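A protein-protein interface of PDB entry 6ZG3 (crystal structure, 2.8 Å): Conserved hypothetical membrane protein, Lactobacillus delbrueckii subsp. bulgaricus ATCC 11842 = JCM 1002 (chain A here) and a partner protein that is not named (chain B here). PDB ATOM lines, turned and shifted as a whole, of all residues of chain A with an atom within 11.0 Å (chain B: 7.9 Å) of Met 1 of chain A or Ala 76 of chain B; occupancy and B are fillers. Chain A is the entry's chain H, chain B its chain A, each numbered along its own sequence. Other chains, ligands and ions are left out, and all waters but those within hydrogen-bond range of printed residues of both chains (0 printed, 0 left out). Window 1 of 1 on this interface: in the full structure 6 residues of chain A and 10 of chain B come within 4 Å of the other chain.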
ATOM      1  N   MET A   1      16.810  28.710 -11.759  1.00  0.00           N
ATOM      2  CA  MET A   1      16.296  28.259 -10.467  1.00  0.00           C
ATOM      3  C   MET A   1      16.797  29.139  -9.302  1.00  0.00           C
ATOM      4  O   MET A   1      16.676  28.751  -8.139  1.00  0.00           O
ATOM      5  CB  MET A   1      16.670  26.783 -10.201  1.00  0.00           C
ATOM      6  CG  MET A   1      16.534  25.827 -11.391  1.00  0.00           C
ATOM      7  SD  MET A   1      14.885  25.122 -11.619  1.00  0.00           S
ATOM      8  CE  MET A   1      14.601  24.387 -10.012  1.00  0.00           C
ATOM      9  N   TYR A   2      17.392  30.294  -9.590  1.00  0.00           N
ATOM     10  CA  TYR A   2      17.763  31.237  -8.542  1.00  0.00           C
ATOM     11  C   TYR A   2      16.979  32.506  -8.816  1.00  0.00           C
ATOM     12  O   TYR A   2      17.084  33.080  -9.906  1.00  0.00           O
ATOM     13  CB  TYR A   2      19.267  31.531  -8.493  1.00  0.00           C
ATOM     14  CG  TYR A   2      20.066  30.493  -7.753  1.00  0.00           C
ATOM     15  CD1 TYR A   2      19.467  29.695  -6.813  1.00  0.00           C
ATOM     16  CD2 TYR A   2      21.412  30.291  -8.017  1.00  0.00           C
ATOM     17  CE1 TYR A   2      20.176  28.726  -6.144  1.00  0.00           C
ATOM     18  CE2 TYR A   2      22.142  29.313  -7.354  1.00  0.00           C
ATOM     19  CZ  TYR A   2      21.511  28.530  -6.410  1.00  0.00           C
ATOM     20  OH  TYR A   2      22.178  27.538  -5.713  1.00  0.00           O
ATOM     21  N   ASP A   3      16.246  32.960  -7.803  1.00  0.00           N
ATOM     22  CA  ASP A   3      15.388  34.142  -7.868  1.00  0.00           C
ATOM     23  C   ASP A   3      14.466  34.053  -9.086  1.00  0.00           C
ATOM     24  O   ASP A   3      14.460  34.913  -9.969  1.00  0.00           O
ATOM     25  CB  ASP A   3      16.223  35.421  -7.900  1.00  0.00           C
ATOM     26  CG  ASP A   3      15.615  36.523  -7.068  1.00  0.00           C
ATOM     27  OD1 ASP A   3      14.675  37.185  -7.542  1.00  0.00           O
ATOM     28  OD2 ASP A   3      16.104  36.739  -5.936  1.00  0.00           O
ATOM     29  N   SER A   4      13.663  32.982  -9.096  1.00  0.00           N
ATOM     30  CA  SER A   4      12.898  32.609 -10.285  1.00  0.00           C
ATOM     31  C   SER A   4      11.895  33.686 -10.661  1.00  0.00           C
ATOM     32  O   SER A   4      11.719  34.008 -11.848  1.00  0.00           O
ATOM     33  CB  SER A   4      12.188  31.286 -10.046  1.00  0.00           C
ATOM     34  OG  SER A   4      11.445  31.388  -8.850  1.00  0.00           O
ATOM     35  N   GLU A   5      11.195  34.229  -9.662  1.00  0.00           N
ATOM     36  CA  GLU A   5      10.219  35.267  -9.947  1.00  0.00           C
ATOM     37  C   GLU A   5      10.872  36.482 -10.599  1.00  0.00           C
ATOM     38  O   GLU A   5      10.243  37.130 -11.439  1.00  0.00           O
ATOM     39  CB  GLU A   5       9.463  35.653  -8.673  1.00  0.00           C
ATOM     40  CG  GLU A   5       8.378  34.622  -8.293  1.00  0.00           C
ATOM     41  CD  GLU A   5       7.284  35.177  -7.366  1.00  0.00           C
ATOM     42  OE1 GLU A   5       7.406  36.357  -6.963  1.00  0.00           O
ATOM     43  OE2 GLU A   5       6.309  34.436  -7.036  1.00  0.00           O
ATOM     44  N   ALA A   6      12.146  36.769 -10.291  1.00  0.00           N
ATOM     45  CA  ALA A   6      12.831  37.864 -10.985  1.00  0.00           C
ATOM     46  C   ALA A   6      13.175  37.496 -12.423  1.00  0.00           C
ATOM     47  O   ALA A   6      13.061  38.338 -13.326  1.00  0.00           O
ATOM     48  CB  ALA A   6      14.095  38.284 -10.241  1.00  0.00           C
ATOM     49  N   ARG A   7      13.617  36.254 -12.656  1.00  0.00           N
ATOM     50  CA  ARG A   7      13.854  35.813 -14.023  1.00  0.00           C
ATOM     51  C   ARG A   7      12.617  36.070 -14.862  1.00  0.00           C
ATOM     52  O   ARG A   7      12.674  36.770 -15.885  1.00  0.00           O
ATOM     53  CB  ARG A   7      14.222  34.322 -14.058  1.00  0.00           C
ATOM     54  CG  ARG A   7      15.721  33.970 -14.176  1.00  0.00           C
ATOM     55  CD  ARG A   7      15.924  32.453 -14.437  1.00  0.00           C
ATOM     56  NE  ARG A   7      15.258  31.580 -13.455  1.00  0.00           N
ATOM     57  CZ  ARG A   7      14.560  30.480 -13.748  1.00  0.00           C
ATOM     58  NH1 ARG A   7      14.388  30.104 -15.012  1.00  0.00           N
ATOM     59  NH2 ARG A   7      14.015  29.766 -12.769  1.00  0.00           N
ATOM     60  N   GLN A   8      11.467  35.583 -14.377  1.00  0.00           N
ATOM     61  CA  GLN A   8      10.229  35.682 -15.144  1.00  0.00           C
ATOM     62  C   GLN A   8       9.739  37.127 -15.238  1.00  0.00           C
ATOM     63  O   GLN A   8       9.252  37.544 -16.291  1.00  0.00           O
ATOM     64  CB  GLN A   8       9.150  34.782 -14.529  1.00  0.00           C
ATOM     65  CG  GLN A   8       8.069  34.290 -15.527  1.00  0.00           C
ATOM     66  CD  GLN A   8       8.554  33.134 -16.425  1.00  0.00           C
ATOM     67  OE1 GLN A   8       9.363  32.295 -16.000  1.00  0.00           O
ATOM     68  NE2 GLN A   8       8.061  33.093 -17.667  1.00  0.00           N
ATOM     69  N   ARG A 206      13.761  26.502 -23.214  1.00  0.00           N
ATOM     70  CA  ARG A 206      14.495  26.690 -21.960  1.00  0.00           C
ATOM     71  C   ARG A 206      14.007  27.911 -21.175  1.00  0.00           C
ATOM     72  O   ARG A 206      13.720  28.967 -21.752  1.00  0.00           O
ATOM     73  CB  ARG A 206      15.998  26.843 -22.223  1.00  0.00           C
ATOM     74  CG  ARG A 206      16.515  26.078 -23.420  1.00  0.00           C
ATOM     75  CD  ARG A 206      16.540  26.935 -24.684  1.00  0.00           C
ATOM     76  NE  ARG A 206      17.893  27.344 -25.055  1.00  0.00           N
ATOM     77  CZ  ARG A 206      18.836  26.527 -25.532  1.00  0.00           C
ATOM     78  NH1 ARG A 206      18.595  25.226 -25.695  1.00  0.00           N
ATOM     79  NH2 ARG A 206      20.035  27.014 -25.837  1.00  0.00           N
ATOM     80  N   ARG A 207      13.962  27.765 -19.845  1.00  0.00           N
ATOM     81  CA  ARG A 207      13.485  28.802 -18.912  1.00  0.00           C
ATOM     82  C   ARG A 207      12.082  29.299 -19.255  1.00  0.00           C
ATOM     83  O   ARG A 207      11.297  29.622 -18.360  1.00  0.00           O
ATOM     84  CB  ARG A 207      14.455  29.993 -18.857  1.00  0.00           C
ATOM     85  CG  ARG A 207      13.780  31.386 -18.854  1.00  0.00           C
ATOM     86  CD  ARG A 207      14.774  32.506 -18.554  1.00  0.00           C
ATOM     87  NE  ARG A 207      15.256  33.227 -19.735  1.00  0.00           N
ATOM     88  CZ  ARG A 207      16.225  32.800 -20.548  1.00  0.00           C
ATOM     89  NH1 ARG A 207      16.833  31.638 -20.316  1.00  0.00           N
ATOM     90  NH2 ARG A 207      16.599  33.544 -21.590  1.00  0.00           N
ATOM     91  N   VAL B  29      29.583  20.126 -10.473  1.00  0.00           N
ATOM     92  CA  VAL B  29      28.405  20.740 -11.068  1.00  0.00           C
ATOM     93  C   VAL B  29      27.863  19.793 -12.135  1.00  0.00           C
ATOM     94  O   VAL B  29      28.576  19.422 -13.073  1.00  0.00           O
ATOM     95  CB  VAL B  29      28.736  22.130 -11.644  1.00  0.00           C
ATOM     96  CG1 VAL B  29      27.573  22.681 -12.429  1.00  0.00           C
ATOM     97  CG2 VAL B  29      29.081  23.123 -10.527  1.00  0.00           C
ATOM     98  N   THR B  30      26.609  19.385 -11.989  1.00  0.00           N
ATOM     99  CA  THR B  30      25.903  18.735 -13.080  1.00  0.00           C
ATOM    100  C   THR B  30      24.691  19.585 -13.429  1.00  0.00           C
ATOM    101  O   THR B  30      24.093  20.223 -12.552  1.00  0.00           O
ATOM    102  CB  THR B  30      25.454  17.317 -12.751  1.00  0.00           C
ATOM    103  OG1 THR B  30      24.423  17.374 -11.763  1.00  0.00           O
ATOM    104  CG2 THR B  30      26.604  16.516 -12.214  1.00  0.00           C
ATOM    105  N   PHE B  31      24.384  19.642 -14.722  1.00  0.00           N
ATOM    106  CA  PHE B  31      23.320  20.495 -15.224  1.00  0.00           C
ATOM    107  C   PHE B  31      22.705  19.832 -16.442  1.00  0.00           C
ATOM    108  O   PHE B  31      23.415  19.529 -17.402  1.00  0.00           O
ATOM    109  CB  PHE B  31      23.855  21.890 -15.578  1.00  0.00           C
ATOM    110  CG  PHE B  31      22.817  22.812 -16.148  1.00  0.00           C
ATOM    111  CD1 PHE B  31      21.997  23.527 -15.309  1.00  0.00           C
ATOM    112  CD2 PHE B  31      22.642  22.936 -17.518  1.00  0.00           C
ATOM    113  CE1 PHE B  31      21.029  24.354 -15.820  1.00  0.00           C
ATOM    114  CE2 PHE B  31      21.663  23.767 -18.034  1.00  0.00           C
ATOM    115  CZ  PHE B  31      20.856  24.474 -17.180  1.00  0.00           C
ATOM    116  N   THR B  32      21.394  19.631 -16.421  1.00  0.00           N
ATOM    117  CA  THR B  32      20.656  19.160 -17.585  1.00  0.00           C
ATOM    118  C   THR B  32      19.745  20.297 -18.029  1.00  0.00           C
ATOM    119  O   THR B  32      18.960  20.802 -17.221  1.00  0.00           O
ATOM    120  CB  THR B  32      19.802  17.939 -17.256  1.00  0.00           C
ATOM    121  OG1 THR B  32      18.731  18.366 -16.412  1.00  0.00           O
ATOM    122  CG2 THR B  32      20.575  16.880 -16.522  1.00  0.00           C
ATOM    123  N   PRO B  34      16.498  21.926 -19.210  1.00  0.00           N
ATOM    124  CA  PRO B  34      15.224  21.344 -18.775  1.00  0.00           C
ATOM    125  C   PRO B  34      14.596  20.465 -19.833  1.00  0.00           C
ATOM    126  O   PRO B  34      14.202  19.328 -19.549  1.00  0.00           O
ATOM    127  CB  PRO B  34      14.367  22.584 -18.465  1.00  0.00           C
ATOM    128  CG  PRO B  34      15.330  23.728 -18.386  1.00  0.00           C
ATOM    129  CD  PRO B  34      16.414  23.386 -19.345  1.00  0.00           C
ATOM    130  N   THR B  66      27.285  26.586 -21.156  1.00  0.00           N
ATOM    131  CA  THR B  66      26.503  26.547 -19.940  1.00  0.00           C
ATOM    132  C   THR B  66      27.242  27.120 -18.735  1.00  0.00           C
ATOM    133  O   THR B  66      26.601  27.486 -17.752  1.00  0.00           O
ATOM    134  CB  THR B  66      26.077  25.087 -19.717  1.00  0.00           C
ATOM    135  OG1 THR B  66      24.917  24.820 -20.517  1.00  0.00           O
ATOM    136  CG2 THR B  66      25.759  24.772 -18.294  1.00  0.00           C
ATOM    137  N   LYS B  69      26.622  31.289 -17.490  1.00  0.00           N
ATOM    138  CA  LYS B  69      25.353  31.457 -16.800  1.00  0.00           C
ATOM    139  C   LYS B  69      25.257  30.612 -15.536  1.00  0.00           C
ATOM    140  O   LYS B  69      24.376  30.870 -14.723  1.00  0.00           O
ATOM    141  CB  LYS B  69      24.179  31.164 -17.733  1.00  0.00           C
ATOM    142  CG  LYS B  69      24.112  32.087 -18.942  1.00  0.00           C
ATOM    143  CD  LYS B  69      22.976  31.660 -19.866  1.00  0.00           C
ATOM    144  CE  LYS B  69      22.848  32.564 -21.096  1.00  0.00           C
ATOM    145  NZ  LYS B  69      21.475  32.480 -21.702  1.00  0.00           N
ATOM    146  N   LEU B  70      26.129  29.622 -15.332  1.00  0.00           N
ATOM    147  CA  LEU B  70      26.165  28.950 -14.030  1.00  0.00           C
ATOM    148  C   LEU B  70      27.038  29.682 -13.015  1.00  0.00           C
ATOM    149  O   LEU B  70      26.729  29.697 -11.813  1.00  0.00           O
ATOM    150  CB  LEU B  70      26.677  27.515 -14.160  1.00  0.00           C
ATOM    151  CG  LEU B  70      25.689  26.396 -14.375  1.00  0.00           C
ATOM    152  CD1 LEU B  70      26.428  25.301 -15.036  1.00  0.00           C
ATOM    153  CD2 LEU B  70      25.146  25.935 -13.057  1.00  0.00           C
ATOM    154  N   GLY B  73      24.878  32.615 -11.816  1.00  0.00           N
ATOM    155  CA  GLY B  73      23.659  32.225 -11.129  1.00  0.00           C
ATOM    156  C   GLY B  73      22.424  32.066 -11.999  1.00  0.00           C
ATOM    157  O   GLY B  73      21.447  31.449 -11.547  1.00  0.00           O
ATOM    158  N   LEU B  74      22.424  32.596 -13.228  1.00  0.00           N
ATOM    159  CA  LEU B  74      21.258  32.492 -14.109  1.00  0.00           C
ATOM    160  C   LEU B  74      20.752  31.058 -14.257  1.00  0.00           C
ATOM    161  O   LEU B  74      19.548  30.842 -14.450  1.00  0.00           O
ATOM    162  CB  LEU B  74      21.595  33.063 -15.478  1.00  0.00           C
ATOM    163  CG  LEU B  74      22.018  34.525 -15.375  1.00  0.00           C
ATOM    164  CD1 LEU B  74      22.099  35.218 -16.741  1.00  0.00           C
ATOM    165  CD2 LEU B  74      21.088  35.262 -14.452  1.00  0.00           C
ATOM    166  N   LEU B  75      21.643  30.077 -14.225  1.00  0.00           N
ATOM    167  CA  LEU B  75      21.267  28.674 -14.203  1.00  0.00           C
ATOM    168  C   LEU B  75      21.678  28.096 -12.853  1.00  0.00           C
ATOM    169  O   LEU B  75      22.745  28.420 -12.336  1.00  0.00           O
ATOM    170  CB  LEU B  75      21.960  27.886 -15.313  1.00  0.00           C
ATOM    171  CG  LEU B  75      21.603  28.280 -16.733  1.00  0.00           C
ATOM    172  CD1 LEU B  75      22.438  27.469 -17.687  1.00  0.00           C
ATOM    173  CD2 LEU B  75      20.147  28.044 -16.962  1.00  0.00           C
ATOM    174  N   ALA B  76      20.841  27.259 -12.280  1.00  0.00           N
ATOM    175  CA  ALA B  76      21.241  26.544 -11.089  1.00  0.00           C
ATOM    176  C   ALA B  76      21.840  25.214 -11.473  1.00  0.00           C
ATOM    177  O   ALA B  76      21.715  24.759 -12.611  1.00  0.00           O
ATOM    178  CB  ALA B  76      20.059  26.340 -10.174  1.00  0.00           C
ATOM    179  N   PRO B  77      22.534  24.570 -10.554  1.00  0.00           N
ATOM    180  CA  PRO B  77      22.883  23.160 -10.770  1.00  0.00           C
ATOM    181  C   PRO B  77      21.680  22.246 -10.591  1.00  0.00           C
ATOM    182  O   PRO B  77      20.552  22.710 -10.437  1.00  0.00           O
ATOM    183  CB  PRO B  77      23.967  22.910  -9.719  1.00  0.00           C
ATOM    184  CG  PRO B  77      24.588  24.235  -9.545  1.00  0.00           C
ATOM    185  CD  PRO B  77      23.446  25.204  -9.591  1.00  0.00           C
ATOM    186  N   ASP B  78      21.907  20.943 -10.622  1.00  0.00           N
ATOM    187  CA  ASP B  78      20.806  20.007 -10.545  1.00  0.00           C
ATOM    188  C   ASP B  78      20.580  19.545  -9.116  1.00  0.00           C
ATOM    189  O   ASP B  78      19.431  19.431  -8.672  1.00  0.00           O
ATOM    190  CB  ASP B  78      21.068  18.812 -11.475  1.00  0.00           C
ATOM    191  CG  ASP B  78      20.968  19.179 -12.957  1.00  0.00           C
ATOM    192  OD1 ASP B  78      20.621  20.343 -13.264  1.00  0.00           O
ATOM    193  OD2 ASP B  78      21.216  18.297 -13.814  1.00  0.00           O
ATOM    194  N   ASP B  79      21.660  19.334  -8.370  1.00  0.00           N
ATOM    195  CA  ASP B  79      21.590  18.877  -6.986  1.00  0.00           C
ATOM    196  C   ASP B  79      22.422  19.824  -6.137  1.00  0.00           C
ATOM    197  O   ASP B  79      23.605  19.559  -5.911  1.00  0.00           O
ATOM    198  CB  ASP B  79      22.087  17.448  -6.880  1.00  0.00           C
ATOM    199  CG  ASP B  79      21.960  16.893  -5.487  1.00  0.00           C
ATOM    200  OD1 ASP B  79      21.309  17.550  -4.657  1.00  0.00           O
ATOM    201  OD2 ASP B  79      22.501  15.794  -5.230  1.00  0.00           O
ATOM    202  N   LEU B  80      21.789  20.889  -5.626  1.00  0.00           N
ATOM    203  CA  LEU B  80      22.481  21.910  -4.831  1.00  0.00           C
ATOM    204  C   LEU B  80      23.102  21.338  -3.565  1.00  0.00           C
ATOM    205  O   LEU B  80      23.907  22.021  -2.921  1.00  0.00           O
ATOM    206  CB  LEU B  80      21.534  23.050  -4.444  1.00  0.00           C
ATOM    207  CG  LEU B  80      20.800  23.899  -5.487  1.00  0.00           C
ATOM    208  CD1 LEU B  80      21.750  24.396  -6.578  1.00  0.00           C
ATOM    209  CD2 LEU B  80      19.581  23.173  -6.072  1.00  0.00           C
ATOM    210  N   SER B  83      26.628  19.919  -5.382  1.00  0.00           N
ATOM    211  CA  SER B  83      27.474  20.833  -6.128  1.00  0.00           C
ATOM    212  C   SER B  83      27.699  22.093  -5.311  1.00  0.00           C
ATOM    213  O   SER B  83      27.015  22.337  -4.314  1.00  0.00           O
ATOM    214  CB  SER B  83      26.842  21.215  -7.474  1.00  0.00           C
ATOM    215  OG  SER B  83      25.851  20.280  -7.897  1.00  0.00           O
ATOM    216  N   ILE B  85      29.345  26.166  -6.397  1.00  0.00           N
ATOM    217  CA  ILE B  85      30.154  27.189  -7.043  1.00  0.00           C
ATOM    218  C   ILE B  85      30.535  28.230  -5.995  1.00  0.00           C
ATOM    219  O   ILE B  85      29.780  28.481  -5.050  1.00  0.00           O
ATOM    220  CB  ILE B  85      29.379  27.814  -8.214  1.00  0.00           C
ATOM    221  CG1 ILE B  85      29.125  26.763  -9.295  1.00  0.00           C
ATOM    222  CG2 ILE B  85      30.083  29.044  -8.753  1.00  0.00           C
ATOM    223  CD1 ILE B  85      28.107  27.213 -10.313  1.00  0.00           C
ATOM    224  N   LEU B  92      27.863  30.603  -4.109  1.00  0.00           N
ATOM    225  CA  LEU B  92      26.705  30.952  -4.925  1.00  0.00           C
ATOM    226  C   LEU B  92      25.503  30.204  -4.396  1.00  0.00           C
ATOM    227  O   LEU B  92      25.511  28.973  -4.337  1.00  0.00           O
ATOM    228  CB  LEU B  92      26.930  30.628  -6.399  1.00  0.00           C
ATOM    229  CG  LEU B  92      25.867  31.279  -7.291  1.00  0.00           C
ATOM    230  CD1 LEU B  92      25.493  32.617  -6.775  1.00  0.00           C
ATOM    231  CD2 LEU B  92      26.320  31.446  -8.708  1.00  0.00           C
ATOM    232  N   GLY B  93      24.491  30.950  -3.977  1.00  0.00           N
ATOM    233  CA  GLY B  93      23.311  30.392  -3.357  1.00  0.00           C
ATOM    234  C   GLY B  93      22.145  31.310  -3.609  1.00  0.00           C
ATOM    235  O   GLY B  93      22.284  32.266  -4.366  1.00  0.00           O
ATOM    236  N   ALA B  94      21.009  31.049  -2.966  1.00  0.00           N
ATOM    237  CA  ALA B  94      19.819  31.868  -3.175  1.00  0.00           C
ATOM    238  C   ALA B  94      20.008  33.286  -2.649  1.00  0.00           C
ATOM    239  O   ALA B  94      19.673  34.268  -3.323  1.00  0.00           O
ATOM    240  CB  ALA B  94      18.633  31.201  -2.501  1.00  0.00           C
ATOM    241  N   VAL B  97      23.027  35.455  -4.820  1.00  0.00           N
ATOM    242  CA  VAL B  97      23.071  35.557  -6.277  1.00  0.00           C
ATOM    243  C   VAL B  97      23.499  36.947  -6.711  1.00  0.00           C
ATOM    244  O   VAL B  97      24.359  37.115  -7.586  1.00  0.00           O
ATOM    245  CB  VAL B  97      21.696  35.221  -6.869  1.00  0.00           C
ATOM    246  CG1 VAL B  97      21.728  35.424  -8.332  1.00  0.00           C
ATOM    247  CG2 VAL B  97      21.365  33.829  -6.592  1.00  0.00           C
ATOM    248  N   ARG B 101      26.809  38.368  -8.504  1.00  0.00           N
ATOM    249  CA  ARG B 101      26.790  39.034  -9.807  1.00  0.00           C
ATOM    250  C   ARG B 101      27.534  40.367  -9.778  1.00  0.00           C
ATOM    251  O   ARG B 101      27.987  40.836 -10.828  1.00  0.00           O
ATOM    252  CB  ARG B 101      25.351  39.233 -10.304  1.00  0.00           C
ATOM    253  CG  ARG B 101      24.599  37.911 -10.513  1.00  0.00           C
ATOM    254  CD  ARG B 101      23.169  38.040 -11.052  1.00  0.00           C
ATOM    255  NE  ARG B 101      22.464  36.753 -11.013  1.00  0.00           N
ATOM    256  CZ  ARG B 101      21.180  36.554 -11.348  1.00  0.00           C
ATOM    257  NH1 ARG B 101      20.408  37.554 -11.778  1.00  0.00           N
ATOM    258  NH2 ARG B 101      20.671  35.326 -11.271  1.00  0.00           N
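O of Lys 69 of chain B sits at hydrogen-bond distance from N of Leu 74 of chain B (3.0 Å).
The backbone carbonyl oxygen (O) of Ile 85 of chain B is in hydrogen-bond range of the backbone NH (N) of Leu 92 of chain B, at 3.0 Å.
Of chain A, only Met 1 (3.4 Å) comes within 4 Å of Ala 76 of chain B.
No residue of chain A comes within 4 Å of Leu 70 of chain B.
No residue of chain A comes within 4 Å of Leu 75 of chain B.
No residue of chain A comes within 4 Å of Pro 77 of chain B.
No residue of chain A comes within 4 Å of Asp 78 of chain B.
Of the printed residues of chain B, Arg 7 of chain A touches Leu 74 (3.97 Å).
Of the printed residues of chain A, Gly 93 of chain B touches Tyr 2 (3.9 Å).
Of the printed residues of chain A, Leu 74 of chain B touches Arg 7.
Of the printed residues of chain A, Leu 92 of chain B touches Tyr 2.
Of the printed residues of chain A, Val 97 of chain B touches Tyr 2 (3.6 Å).
The nearest residue of chain B that does not touch Met 1 of chain A is Leu 74 of chain B (4.4 Å).
The nearest residue of chain A that does not touch Ala 76 of chain B is Tyr 2 of chain A (4.6 Å).
Of the 23 printed residues of chain B, 7 touch a printed residue of chain A.
Printed residues of chain A that touch a printed residue of chain B: Met 1, Tyr 2 and Arg 7.
Among the printed residues, pairs that only touch across the chains: Tyr 2 of chain A with Leu 80 of chain B, Met 1 of chain A with Ala 76 of chain B, Tyr 2 of chain A with Val 97 of chain B, Tyr 2 of chain A with Gly 73 of chain B, Tyr 2 of chain A with Gly 93 of chain B, Tyr 2 of chain A with Leu 92 of chain B and Arg 7 of chain A with Leu 74 of chain B.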
